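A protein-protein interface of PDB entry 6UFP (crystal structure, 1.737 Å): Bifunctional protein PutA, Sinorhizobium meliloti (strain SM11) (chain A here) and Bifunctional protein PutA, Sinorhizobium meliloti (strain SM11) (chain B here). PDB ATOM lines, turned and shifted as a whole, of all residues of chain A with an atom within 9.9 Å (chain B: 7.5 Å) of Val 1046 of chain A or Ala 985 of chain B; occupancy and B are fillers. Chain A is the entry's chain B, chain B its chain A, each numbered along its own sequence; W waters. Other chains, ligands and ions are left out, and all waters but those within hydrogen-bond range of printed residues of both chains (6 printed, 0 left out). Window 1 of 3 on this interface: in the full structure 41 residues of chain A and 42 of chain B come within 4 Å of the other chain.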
ATOM      1  N   GLN A1042      12.962  30.424  12.927  1.00  0.00           N
ATOM      2  CA  GLN A1042      13.218  30.344  14.368  1.00  0.00           C
ATOM      3  C   GLN A1042      11.983  29.985  15.190  1.00  0.00           C
ATOM      4  O   GLN A1042      11.998  30.123  16.420  1.00  0.00           O
ATOM      5  CB  GLN A1042      13.828  31.653  14.895  1.00  0.00           C
ATOM      6  CG  GLN A1042      15.192  31.972  14.291  1.00  0.00           C
ATOM      7  CD  GLN A1042      15.707  33.342  14.701  1.00  0.00           C
ATOM      8  OE1 GLN A1042      15.033  34.355  14.518  1.00  0.00           O
ATOM      9  NE2 GLN A1042      16.897  33.372  15.273  1.00  0.00           N
ATOM     10  N   HIS A1043      10.912  29.522  14.560  1.00  0.00           N
ATOM     11  CA  HIS A1043       9.641  29.314  15.257  1.00  0.00           C
ATOM     12  C   HIS A1043       9.592  27.876  15.755  1.00  0.00           C
ATOM     13  O   HIS A1043       9.178  26.961  15.046  1.00  0.00           O
ATOM     14  CB  HIS A1043       8.478  29.644  14.329  1.00  0.00           C
ATOM     15  CG  HIS A1043       7.123  29.496  14.952  1.00  0.00           C
ATOM     16  ND1 HIS A1043       6.463  30.544  15.556  1.00  0.00           N
ATOM     17  CD2 HIS A1043       6.281  28.435  15.020  1.00  0.00           C
ATOM     18  CE1 HIS A1043       5.287  30.130  15.997  1.00  0.00           C
ATOM     19  NE2 HIS A1043       5.147  28.856  15.673  1.00  0.00           N
ATOM     20  N   SER A1044      10.036  27.674  16.992  1.00  0.00           N
ATOM     21  CA  SER A1044       9.978  26.364  17.631  1.00  0.00           C
ATOM     22  C   SER A1044      10.222  26.580  19.117  1.00  0.00           C
ATOM     23  O   SER A1044      10.590  27.674  19.545  1.00  0.00           O
ATOM     24  CB  SER A1044      11.008  25.393  17.037  1.00  0.00           C
ATOM     25  OG  SER A1044      12.305  25.749  17.472  1.00  0.00           O
ATOM     26  N   SER A1045       9.988  25.534  19.902  1.00  0.00           N
ATOM     27  CA  SER A1045      10.221  25.595  21.340  1.00  0.00           C
ATOM     28  C   SER A1045      10.487  24.192  21.849  1.00  0.00           C
ATOM     29  O   SER A1045       9.831  23.249  21.412  1.00  0.00           O
ATOM     30  CB  SER A1045       9.004  26.187  22.073  1.00  0.00           C
ATOM     31  OG  SER A1045       9.186  26.110  23.485  1.00  0.00           O
ATOM     32  N   VAL A1046      11.443  24.052  22.776  1.00  0.00           N
ATOM     33  CA  VAL A1046      11.730  22.738  23.334  1.00  0.00           C
ATOM     34  C   VAL A1046      10.825  22.407  24.504  1.00  0.00           C
ATOM     35  O   VAL A1046      10.885  21.288  25.025  1.00  0.00           O
ATOM     36  CB  VAL A1046      13.203  22.607  23.776  1.00  0.00           C
ATOM     37  CG1 VAL A1046      14.106  22.816  22.582  1.00  0.00           C
ATOM     38  CG2 VAL A1046      13.524  23.590  24.887  1.00  0.00           C
ATOM     39  N   HIS A1047       9.970  23.334  24.916  1.00  0.00           N
ATOM     40  CA  HIS A1047       9.123  23.120  26.071  1.00  0.00           C
ATOM     41  C   HIS A1047       7.803  22.485  25.664  1.00  0.00           C
ATOM     42  O   HIS A1047       7.253  22.782  24.603  1.00  0.00           O
ATOM     43  CB  HIS A1047       8.916  24.451  26.781  1.00  0.00           C
ATOM     44  CG  HIS A1047      10.215  25.078  27.177  1.00  0.00           C
ATOM     45  ND1 HIS A1047      11.036  24.527  28.142  1.00  0.00           N
ATOM     46  CD2 HIS A1047      10.888  26.139  26.671  1.00  0.00           C
ATOM     47  CE1 HIS A1047      12.133  25.254  28.246  1.00  0.00           C
ATOM     48  NE2 HIS A1047      12.069  26.236  27.364  1.00  0.00           N
ATOM     49  N   THR A1048       7.318  21.580  26.508  1.00  0.00           N
ATOM     50  CA  THR A1048       6.033  20.933  26.295  1.00  0.00           C
ATOM     51  C   THR A1048       5.107  21.271  27.451  1.00  0.00           C
ATOM     52  O   THR A1048       5.480  21.128  28.624  1.00  0.00           O
ATOM     53  CB  THR A1048       6.197  19.416  26.170  1.00  0.00           C
ATOM     54  OG1 THR A1048       7.195  19.144  25.182  1.00  0.00           O
ATOM     55  CG2 THR A1048       4.872  18.784  25.727  1.00  0.00           C
ATOM     56  N   ASP A1049       3.901  21.702  27.118  1.00  0.00           N
ATOM     57  CA  ASP A1049       2.959  22.104  28.152  1.00  0.00           C
ATOM     58  C   ASP A1049       2.610  20.897  29.021  1.00  0.00           C
ATOM     59  O   ASP A1049       2.268  19.835  28.488  1.00  0.00           O
ATOM     60  CB  ASP A1049       1.715  22.705  27.496  1.00  0.00           C
ATOM     61  CG  ASP A1049       0.672  23.132  28.509  1.00  0.00           C
ATOM     62  OD1 ASP A1049      -0.081  22.253  28.979  1.00  0.00           O
ATOM     63  OD2 ASP A1049       0.621  24.335  28.832  1.00  0.00           O
ATOM     64  N   PRO A1050       2.718  21.004  30.352  1.00  0.00           N
ATOM     65  CA  PRO A1050       2.507  19.816  31.192  1.00  0.00           C
ATOM     66  C   PRO A1050       1.067  19.328  31.194  1.00  0.00           C
ATOM     67  O   PRO A1050       0.825  18.136  31.413  1.00  0.00           O
ATOM     68  CB  PRO A1050       2.946  20.293  32.582  1.00  0.00           C
ATOM     69  CG  PRO A1050       2.730  21.758  32.561  1.00  0.00           C
ATOM     70  CD  PRO A1050       3.055  22.194  31.153  1.00  0.00           C
ATOM     71  N   LEU A1053       0.503  17.182  28.236  1.00  0.00           N
ATOM     72  CA  LEU A1053       1.032  15.856  28.519  1.00  0.00           C
ATOM     73  C   LEU A1053       0.045  15.031  29.336  1.00  0.00           C
ATOM     74  O   LEU A1053      -0.170  13.848  29.049  1.00  0.00           O
ATOM     75  CB  LEU A1053       2.373  15.969  29.250  1.00  0.00           C
ATOM     76  CG  LEU A1053       3.563  16.427  28.392  1.00  0.00           C
ATOM     77  CD1 LEU A1053       4.794  16.654  29.252  1.00  0.00           C
ATOM     78  CD2 LEU A1053       3.866  15.410  27.317  1.00  0.00           C
ATOM     79  N   GLY A1075       1.774  18.894  21.136  1.00  0.00           N
ATOM     80  CA  GLY A1075       2.685  19.299  22.193  1.00  0.00           C
ATOM     81  C   GLY A1075       4.065  19.622  21.660  1.00  0.00           C
ATOM     82  O   GLY A1075       4.679  20.616  22.060  1.00  0.00           O
ATOM     83  N   SER A1076       4.547  18.817  20.708  1.00  0.00           N
ATOM     84  CA  SER A1076       5.869  19.049  20.138  1.00  0.00           C
ATOM     85  C   SER A1076       5.877  20.218  19.167  1.00  0.00           C
ATOM     86  O   SER A1076       6.811  21.026  19.181  1.00  0.00           O
ATOM     87  CB  SER A1076       6.376  17.779  19.446  1.00  0.00           C
ATOM     88  OG  SER A1076       6.611  16.766  20.409  1.00  0.00           O
ATOM     89  N   SER A1077       4.860  20.335  18.311  1.00  0.00           N
ATOM     90  CA  SER A1077       4.949  21.362  17.281  1.00  0.00           C
ATOM     91  C   SER A1077       4.601  22.752  17.811  1.00  0.00           C
ATOM     92  O   SER A1077       4.916  23.749  17.147  1.00  0.00           O
ATOM     93  CB  SER A1077       4.061  21.007  16.091  1.00  0.00           C
ATOM     94  OG  SER A1077       2.707  20.984  16.458  1.00  0.00           O
ATOM     95  N   SER A1078       3.989  22.831  18.992  1.00  0.00           N
ATOM     96  CA  SER A1078       3.703  24.123  19.613  1.00  0.00           C
ATOM     97  C   SER A1078       4.987  24.917  19.825  1.00  0.00           C
ATOM     98  O   SER A1078       6.015  24.372  20.241  1.00  0.00           O
ATOM     99  CB  SER A1078       3.001  23.914  20.962  1.00  0.00           C
ATOM    100  OG  SER A1078       2.869  25.149  21.660  1.00  0.00           O
ATOM    101  N   ALA A1079       4.934  26.211  19.524  1.00  0.00           N
ATOM    102  CA  ALA A1079       6.057  27.096  19.793  1.00  0.00           C
ATOM    103  C   ALA A1079       5.877  27.864  21.095  1.00  0.00           C
ATOM    104  O   ALA A1079       6.606  28.829  21.342  1.00  0.00           O
ATOM    105  CB  ALA A1079       6.274  28.059  18.623  1.00  0.00           C
ATOM    106  N   LEU A1080       4.918  27.459  21.931  1.00  0.00           N
ATOM    107  CA  LEU A1080       4.790  28.043  23.262  1.00  0.00           C
ATOM    108  C   LEU A1080       6.122  27.967  24.002  1.00  0.00           C
ATOM    109  O   LEU A1080       6.729  26.901  24.102  1.00  0.00           O
ATOM    110  CB  LEU A1080       3.708  27.305  24.056  1.00  0.00           C
ATOM    111  CG  LEU A1080       3.602  27.723  25.514  1.00  0.00           C
ATOM    112  CD1 LEU A1080       3.010  29.139  25.639  1.00  0.00           C
ATOM    113  CD2 LEU A1080       2.766  26.709  26.276  1.00  0.00           C
ATOM    114  N   GLY A1081       6.567  29.108  24.526  1.00  0.00           N
ATOM    115  CA  GLY A1081       7.815  29.172  25.260  1.00  0.00           C
ATOM    116  C   GLY A1081       9.008  29.624  24.443  1.00  0.00           C
ATOM    117  O   GLY A1081      10.126  29.679  24.987  1.00  0.00           O
ATOM    118  N   LEU A1082       8.818  29.882  23.152  1.00  0.00           N
ATOM    119  CA  LEU A1082       9.858  30.508  22.345  1.00  0.00           C
ATOM    120  C   LEU A1082      10.337  31.791  23.014  1.00  0.00           C
ATOM    121  O   LEU A1082       9.541  32.574  23.532  1.00  0.00           O
ATOM    122  CB  LEU A1082       9.326  30.814  20.937  1.00  0.00           C
ATOM    123  CG  LEU A1082      10.288  31.511  19.960  1.00  0.00           C
ATOM    124  CD1 LEU A1082      11.578  30.727  19.837  1.00  0.00           C
ATOM    125  CD2 LEU A1082       9.632  31.703  18.585  1.00  0.00           C
ATOM    126  N   ASP A1083      11.656  32.009  22.989  1.00  0.00           N
ATOM    127  CA  ASP A1083      12.255  33.150  23.693  1.00  0.00           C
ATOM    128  C   ASP A1083      13.523  33.535  22.930  1.00  0.00           C
ATOM    129  O   ASP A1083      14.555  32.874  23.072  1.00  0.00           O
ATOM    130  CB  ASP A1083      12.536  32.765  25.144  1.00  0.00           C
ATOM    131  CG  ASP A1083      13.077  33.905  25.980  1.00  0.00           C
ATOM    132  OD1 ASP A1083      13.011  35.068  25.542  1.00  0.00           O
ATOM    133  OD2 ASP A1083      13.575  33.619  27.093  1.00  0.00           O
ATOM    134  N   ALA A1123      -1.897  22.449  24.143  1.00  0.00           N
ATOM    135  CA  ALA A1123      -0.499  22.437  23.702  1.00  0.00           C
ATOM    136  C   ALA A1123       0.092  23.834  23.655  1.00  0.00           C
ATOM    137  O   ALA A1123       1.315  23.995  23.787  1.00  0.00           O
ATOM    138  CB  ALA A1123      -0.373  21.804  22.320  1.00  0.00           C
ATOM    139  N   VAL B 161      21.262  18.617  21.028  1.00  0.00           N
ATOM    140  CA  VAL B 161      20.604  18.931  19.766  1.00  0.00           C
ATOM    141  C   VAL B 161      19.270  19.601  20.068  1.00  0.00           C
ATOM    142  O   VAL B 161      18.459  19.061  20.826  1.00  0.00           O
ATOM    143  CB  VAL B 161      20.404  17.645  18.943  1.00  0.00           C
ATOM    144  CG1 VAL B 161      19.544  17.903  17.768  1.00  0.00           C
ATOM    145  CG2 VAL B 161      21.770  17.053  18.529  1.00  0.00           C
ATOM    146  N   ASN B 162      19.016  20.760  19.453  1.00  0.00           N
ATOM    147  CA  ASN B 162      17.687  21.358  19.570  1.00  0.00           C
ATOM    148  C   ASN B 162      16.844  20.697  18.490  1.00  0.00           C
ATOM    149  O   ASN B 162      16.760  21.174  17.356  1.00  0.00           O
ATOM    150  CB  ASN B 162      17.730  22.878  19.437  1.00  0.00           C
ATOM    151  CG  ASN B 162      16.354  23.523  19.659  1.00  0.00           C
ATOM    152  OD1 ASN B 162      15.314  22.865  19.549  1.00  0.00           O
ATOM    153  ND2 ASN B 162      16.350  24.813  19.976  1.00  0.00           N
ATOM    154  N   ASP B 163      16.230  19.558  18.838  1.00  0.00           N
ATOM    155  CA  ASP B 163      15.514  18.780  17.829  1.00  0.00           C
ATOM    156  C   ASP B 163      14.208  19.442  17.390  1.00  0.00           C
ATOM    157  O   ASP B 163      13.739  19.184  16.273  1.00  0.00           O
ATOM    158  CB  ASP B 163      15.264  17.344  18.340  1.00  0.00           C
ATOM    159  CG  ASP B 163      14.695  17.282  19.777  1.00  0.00           C
ATOM    160  OD1 ASP B 163      15.108  18.062  20.669  1.00  0.00           O
ATOM    161  OD2 ASP B 163      13.838  16.403  20.021  1.00  0.00           O
ATOM    162  N   ARG B 164      13.620  20.308  18.217  1.00  0.00           N
ATOM    163  CA  ARG B 164      12.420  21.001  17.762  1.00  0.00           C
ATOM    164  C   ARG B 164      12.775  22.075  16.744  1.00  0.00           C
ATOM    165  O   ARG B 164      12.035  22.293  15.780  1.00  0.00           O
ATOM    166  CB  ARG B 164      11.661  21.615  18.944  1.00  0.00           C
ATOM    167  CG  ARG B 164      11.050  20.608  19.928  1.00  0.00           C
ATOM    168  CD  ARG B 164      10.452  19.391  19.233  1.00  0.00           C
ATOM    169  NE  ARG B 164       9.404  19.726  18.274  1.00  0.00           N
ATOM    170  CZ  ARG B 164       9.094  18.978  17.216  1.00  0.00           C
ATOM    171  NH1 ARG B 164       9.767  17.854  16.967  1.00  0.00           N
ATOM    172  NH2 ARG B 164       8.120  19.360  16.396  1.00  0.00           N
ATOM    173  N   SER B 165      13.904  22.760  16.950  1.00  0.00           N
ATOM    174  CA  SER B 165      14.394  23.715  15.959  1.00  0.00           C
ATOM    175  C   SER B 165      14.717  23.019  14.641  1.00  0.00           C
ATOM    176  O   SER B 165      14.398  23.525  13.556  1.00  0.00           O
ATOM    177  CB  SER B 165      15.643  24.420  16.514  1.00  0.00           C
ATOM    178  OG  SER B 165      16.229  25.257  15.531  1.00  0.00           O
ATOM    179  N   LEU B 976      19.813  11.094  33.309  1.00  0.00           N
ATOM    180  CA  LEU B 976      19.202  11.115  31.990  1.00  0.00           C
ATOM    181  C   LEU B 976      20.315  11.097  30.955  1.00  0.00           C
ATOM    182  O   LEU B 976      21.233  11.925  31.009  1.00  0.00           O
ATOM    183  CB  LEU B 976      18.309  12.351  31.821  1.00  0.00           C
ATOM    184  CG  LEU B 976      17.713  12.546  30.429  1.00  0.00           C
ATOM    185  CD1 LEU B 976      16.729  11.440  30.078  1.00  0.00           C
ATOM    186  CD2 LEU B 976      17.062  13.930  30.331  1.00  0.00           C
ATOM    187  N   THR B 978      20.575  11.447  27.021  1.00  0.00           N
ATOM    188  CA  THR B 978      19.924  11.804  25.774  1.00  0.00           C
ATOM    189  C   THR B 978      20.728  12.925  25.147  1.00  0.00           C
ATOM    190  O   THR B 978      21.409  13.674  25.846  1.00  0.00           O
ATOM    191  CB  THR B 978      18.469  12.249  25.975  1.00  0.00           C
ATOM    192  OG1 THR B 978      17.906  12.605  24.704  1.00  0.00           O
ATOM    193  CG2 THR B 978      18.397  13.464  26.896  1.00  0.00           C
ATOM    194  N   LEU B 980      18.863  14.977  23.058  1.00  0.00           N
ATOM    195  CA  LEU B 980      17.750  15.741  22.490  1.00  0.00           C
ATOM    196  C   LEU B 980      17.235  16.768  23.497  1.00  0.00           C
ATOM    197  O   LEU B 980      16.797  16.401  24.590  1.00  0.00           O
ATOM    198  CB  LEU B 980      16.611  14.811  22.076  1.00  0.00           C
ATOM    199  CG  LEU B 980      17.001  13.718  21.085  1.00  0.00           C
ATOM    200  CD1 LEU B 980      15.799  12.835  20.785  1.00  0.00           C
ATOM    201  CD2 LEU B 980      17.584  14.328  19.807  1.00  0.00           C
ATOM    202  N   ASP B 981      17.251  18.048  23.110  1.00  0.00           N
ATOM    203  CA  ASP B 981      16.857  19.112  24.041  1.00  0.00           C
ATOM    204  C   ASP B 981      15.408  18.973  24.482  1.00  0.00           C
ATOM    205  O   ASP B 981      15.067  19.322  25.618  1.00  0.00           O
ATOM    206  CB  ASP B 981      17.057  20.480  23.392  1.00  0.00           C
ATOM    207  CG  ASP B 981      18.495  20.925  23.378  1.00  0.00           C
ATOM    208  OD1 ASP B 981      19.320  20.301  24.077  1.00  0.00           O
ATOM    209  OD2 ASP B 981      18.794  21.908  22.660  1.00  0.00           O
ATOM    210  N   GLU B 982      14.521  18.548  23.575  1.00  0.00           N
ATOM    211  CA  GLU B 982      13.119  18.433  23.959  1.00  0.00           C
ATOM    212  C   GLU B 982      12.961  17.403  25.063  1.00  0.00           C
ATOM    213  O   GLU B 982      12.167  17.584  25.993  1.00  0.00           O
ATOM    214  CB  GLU B 982      12.253  18.049  22.761  1.00  0.00           C
ATOM    215  CG  GLU B 982      10.782  17.884  23.124  1.00  0.00           C
ATOM    216  CD  GLU B 982       9.992  17.120  22.084  1.00  0.00           C
ATOM    217  OE1 GLU B 982      10.472  16.058  21.625  1.00  0.00           O
ATOM    218  OE2 GLU B 982       8.891  17.587  21.723  1.00  0.00           O
ATOM    219  N   THR B 983      13.725  16.316  24.974  1.00  0.00           N
ATOM    220  CA  THR B 983      13.641  15.276  25.989  1.00  0.00           C
ATOM    221  C   THR B 983      14.247  15.754  27.305  1.00  0.00           C
ATOM    222  O   THR B 983      13.696  15.486  28.384  1.00  0.00           O
ATOM    223  CB  THR B 983      14.326  13.999  25.473  1.00  0.00           C
ATOM    224  OG1 THR B 983      13.611  13.516  24.326  1.00  0.00           O
ATOM    225  CG2 THR B 983      14.330  12.924  26.546  1.00  0.00           C
ATOM    226  N   ILE B 984      15.352  16.502  27.242  1.00  0.00           N
ATOM    227  CA  ILE B 984      15.931  17.055  28.469  1.00  0.00           C
ATOM    228  C   ILE B 984      14.929  17.966  29.156  1.00  0.00           C
ATOM    229  O   ILE B 984      14.711  17.874  30.371  1.00  0.00           O
ATOM    230  CB  ILE B 984      17.246  17.794  28.175  1.00  0.00           C
ATOM    231  CG1 ILE B 984      18.310  16.811  27.701  1.00  0.00           C
ATOM    232  CG2 ILE B 984      17.752  18.481  29.421  1.00  0.00           C
ATOM    233  CD1 ILE B 984      19.559  17.488  27.162  1.00  0.00           C
ATOM    234  N   ALA B 985      14.308  18.860  28.390  1.00  0.00           N
ATOM    235  CA  ALA B 985      13.386  19.822  28.989  1.00  0.00           C
ATOM    236  C   ALA B 985      12.190  19.114  29.609  1.00  0.00           C
ATOM    237  O   ALA B 985      11.778  19.429  30.733  1.00  0.00           O
ATOM    238  CB  ALA B 985      12.932  20.832  27.930  1.00  0.00           C
ATOM    239  N   HIS B 986      11.629  18.143  28.890  1.00  0.00           N
ATOM    240  CA  HIS B 986      10.477  17.400  29.383  1.00  0.00           C
ATOM    241  C   HIS B 986      10.821  16.658  30.667  1.00  0.00           C
ATOM    242  O   HIS B 986      10.158  16.823  31.699  1.00  0.00           O
ATOM    243  CB  HIS B 986      10.010  16.432  28.293  1.00  0.00           C
ATOM    244  CG  HIS B 986       8.950  15.466  28.727  1.00  0.00           C
ATOM    245  ND1 HIS B 986       8.512  14.447  27.910  1.00  0.00           N
ATOM    246  CD2 HIS B 986       8.246  15.355  29.877  1.00  0.00           C
ATOM    247  CE1 HIS B 986       7.584  13.748  28.540  1.00  0.00           C
ATOM    248  NE2 HIS B 986       7.411  14.271  29.740  1.00  0.00           N
ATOM    249  N   VAL B 987      11.873  15.834  30.620  1.00  0.00           N
ATOM    250  CA  VAL B 987      12.179  14.977  31.762  1.00  0.00           C
ATOM    251  C   VAL B 987      12.591  15.814  32.968  1.00  0.00           C
ATOM    252  O   VAL B 987      12.139  15.571  34.093  1.00  0.00           O
ATOM    253  CB  VAL B 987      13.265  13.950  31.394  1.00  0.00           C
ATOM    254  CG1 VAL B 987      13.749  13.226  32.653  1.00  0.00           C
ATOM    255  CG2 VAL B 987      12.708  12.923  30.396  1.00  0.00           C
ATOM    256  N   THR B 988      13.478  16.796  32.767  1.00  0.00           N
ATOM    257  CA  THR B 988      13.977  17.521  33.929  1.00  0.00           C
ATOM    258  C   THR B 988      12.891  18.411  34.527  1.00  0.00           C
ATOM    259  O   THR B 988      12.940  18.726  35.721  1.00  0.00           O
ATOM    260  CB  THR B 988      15.232  18.343  33.597  1.00  0.00           C
ATOM    261  OG1 THR B 988      14.924  19.381  32.666  1.00  0.00           O
ATOM    262  CG2 THR B 988      16.339  17.458  33.030  1.00  0.00           C
ATOM    263  N   SER B 989      11.892  18.798  33.738  1.00  0.00           N
ATOM    264  CA  SER B 989      10.818  19.595  34.316  1.00  0.00           C
ATOM    265  C   SER B 989       9.814  18.740  35.088  1.00  0.00           C
ATOM    266  O   SER B 989       9.173  19.249  36.009  1.00  0.00           O
ATOM    267  CB  SER B 989      10.114  20.422  33.228  1.00  0.00           C
ATOM    268  OG  SER B 989       9.384  19.614  32.322  1.00  0.00           O
ATOM    269  N   ARG B 990       9.704  17.446  34.781  1.00  0.00           N
ATOM    270  CA  ARG B 990       8.709  16.585  35.412  1.00  0.00           C
ATOM    271  C   ARG B 990       9.258  15.718  36.535  1.00  0.00           C
ATOM    272  O   ARG B 990       8.499  15.359  37.439  1.00  0.00           O
ATOM    273  CB  ARG B 990       8.064  15.690  34.354  1.00  0.00           C
ATOM    274  CG  ARG B 990       7.391  16.484  33.258  1.00  0.00           C
ATOM    275  CD  ARG B 990       6.036  16.959  33.719  1.00  0.00           C
ATOM    276  NE  ARG B 990       5.002  16.066  33.217  1.00  0.00           N
ATOM    277  CZ  ARG B 990       3.708  16.201  33.471  1.00  0.00           C
ATOM    278  NH1 ARG B 990       3.283  17.197  34.240  1.00  0.00           N
ATOM    279  NH2 ARG B 990       2.843  15.340  32.947  1.00  0.00           N
ATOM    280  N   ILE B 991      10.551  15.364  36.502  1.00  0.00           N
ATOM    281  CA  ILE B 991      11.141  14.537  37.550  1.00  0.00           C
ATOM    282  C   ILE B 991      11.219  15.326  38.856  1.00  0.00           C
ATOM    283  O   ILE B 991      11.417  16.548  38.868  1.00  0.00           O
ATOM    284  CB  ILE B 991      12.529  14.015  37.119  1.00  0.00           C
ATOM    285  CG1 ILE B 991      12.975  12.860  38.019  1.00  0.00           C
ATOM    286  CG2 ILE B 991      13.570  15.144  37.089  1.00  0.00           C
ATOM    287  CD1 ILE B 991      12.227  11.568  37.736  1.00  0.00           C
HETATM  288  O   HOH W   1       8.281  20.084  22.674  1.00  0.00           O
HETATM  289  O   HOH W   2      13.486  27.289  15.442  1.00  0.00           O
HETATM  290  O   HOH W   3       6.939  16.950  23.749  1.00  0.00           O
HETATM  291  O   HOH W   4      13.431  25.453  19.917  1.00  0.00           O
HETATM  292  O   HOH W   5       6.879  19.699  30.409  1.00  0.00           O
HETATM  293  O   HOH W   6       9.823  19.361  26.245  1.00  0.00           O
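O of Ser 1076 of chain A sits at hydrogen-bond distance from NE of Arg 164 of chain B (3.0 Å). The backbone NH (N) of Ser 165 of chain B lies close to the side-chain hydroxyl (OG) of Ser 1044 of chain A. OG of Ser 1076 of chain A lies within hydrogen-bond range of OE2 of Glu 982 of chain B.
Water W6 lies within hydrogen-bond range of O of Val 1046 of chain A (2.5 Å), OG1 of Thr 1048 of chain A (2.8 Å), O of Glu 982 of chain B (3.0 Å) and N of His 986 of chain B (3.4 Å). Water W3 lies within hydrogen-bond range of OG1 of Thr 1048 of chain A, OE2 of Glu 982 of chain B and OG of Ser 1076 of chain A. Water W5 bridges O of Thr 1048 of chain A (2.7 Å) and OG of Ser 989 of chain B (3.2 Å). Water W4 lies within hydrogen-bond range of the side-chain hydroxyl of Ser 1044 of chain A (2.7 Å), the side-chain amide nitrogen of Asn 162 of chain B (3.0 Å) and the backbone NH of Ser 1045 of chain A (3.4 Å). Water W1 lies within hydrogen-bond range of OE2 of Glu 982 of chain B (2.7 Å), OG1 of Thr 1048 of chain A (2.9 Å) and O of His 1047 of chain A (3.5 Å). Water W2 lies within hydrogen-bond range of OG of Ser 1044 of chain A (2.8 Å), O of Gln 1042 of chain A (3.3 Å) and OG of Ser 165 of chain B (3.4 Å).
Printed residues of chain B within 4 Å of Ser 1045 of chain A: Arg 164 (3.3 Å). Printed residues of chain B within 4 Å of Val 1046 of chain A: Asn 162, Asp 981, Glu 982 and Ala 985. Thr 1048 of chain A touches none of the printed residues of chain B. Of the printed residues of chain B, Ser 1076 of chain A touches Arg 164 (3.0 Å) and Glu 982 (2.8 Å). Of the printed residues of chain B, Ser 1077 of chain A touches Arg 164 (3.9 Å). Leu 1082 of chain A touches none of the printed residues of chain B. Printed residues of chain A within 4 Å of Arg 164 of chain B: Ser 1044, Ser 1045, Ser 1076 and Ser 1077. No residue of chain A comes within 4 Å of Ile 984 of chain B. No residue of chain A comes within 4 Å of Thr 988 of chain B. The nearest residue of chain B that does not touch Val 1046 of chain A is Arg 164 of chain B (4.1 Å). The nearest printed residue of chain B that does not touch Ser 1044 of chain A is Asn 162 of chain B (4.7 Å).
Arg 164 of chain B touches Ser 1044 of chain A (O to CB, 3.5 Å). Arg 164 of chain B touches Ser 1045 of chain A (CG to O, 3.3 Å). Asn 162 of chain B touches Val 1046 of chain A. CG1 of Val 1046 of chain A touches CB of Asp 981 of chain B, 3.8 Å away. Glu 982 of chain B touches Val 1046 of chain A (CA to O, 3.8 Å). Ala 985 of chain B touches Val 1046 of chain A (CB to O, 3.6 Å). Pro 1050 of chain A touches Arg 990 of chain B. CD1 of Leu 1053 of chain A touches NE2 of His 986 of chain B, 3.6 Å away. Arg 990 of chain B touches Leu 1053 of chain A (NH2 to CB, 3.8 Å). Ser 1077 of chain A touches Arg 164 of chain B.
Hydrophobic or aromatic side chains of chain A within 4 Å of the printed part of chain B: Val 1046, Pro 1050 and Leu 1053. Of the 19 printed residues of chain B, 8 touch a printed residue of chain A. Hydrophobic or aromatic side chains of chain B that line the printed part of chain A: Ala 985 and His 986. Along chain B the printed residues that touch a printed residue of chain A span positions 162 to 990. Among the printed residues, 13 pairs touch across the chains.
OD1 of Asn 162 of chain B lies close to N of Arg 164 of chain B (3.3 Å). The backbone carbonyl oxygen (O) of His 986 of chain B is in hydrogen-bond range of the side-chain hydroxyl (OG) of Ser 989 of chain B (3.0 Å). OG of Ser 1045 of chain A lies within hydrogen-bond range of N of His 1047 of chain A (3.2 Å). OD1 of Asp 163 of chain B lies within hydrogen-bond range of N of Asp 981 of chain B (3.2 Å). The side-chain hydroxyl of Ser 1045 of chain A lies within hydrogen-bond range of the backbone carbonyl oxygen of Leu 1080 of chain A (2.7 Å). The backbone carbonyl oxygen of Ala 985 of chain B sits at hydrogen-bond distance from the side-chain hydroxyl of Ser 989 of chain B, 2.9 Å away.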
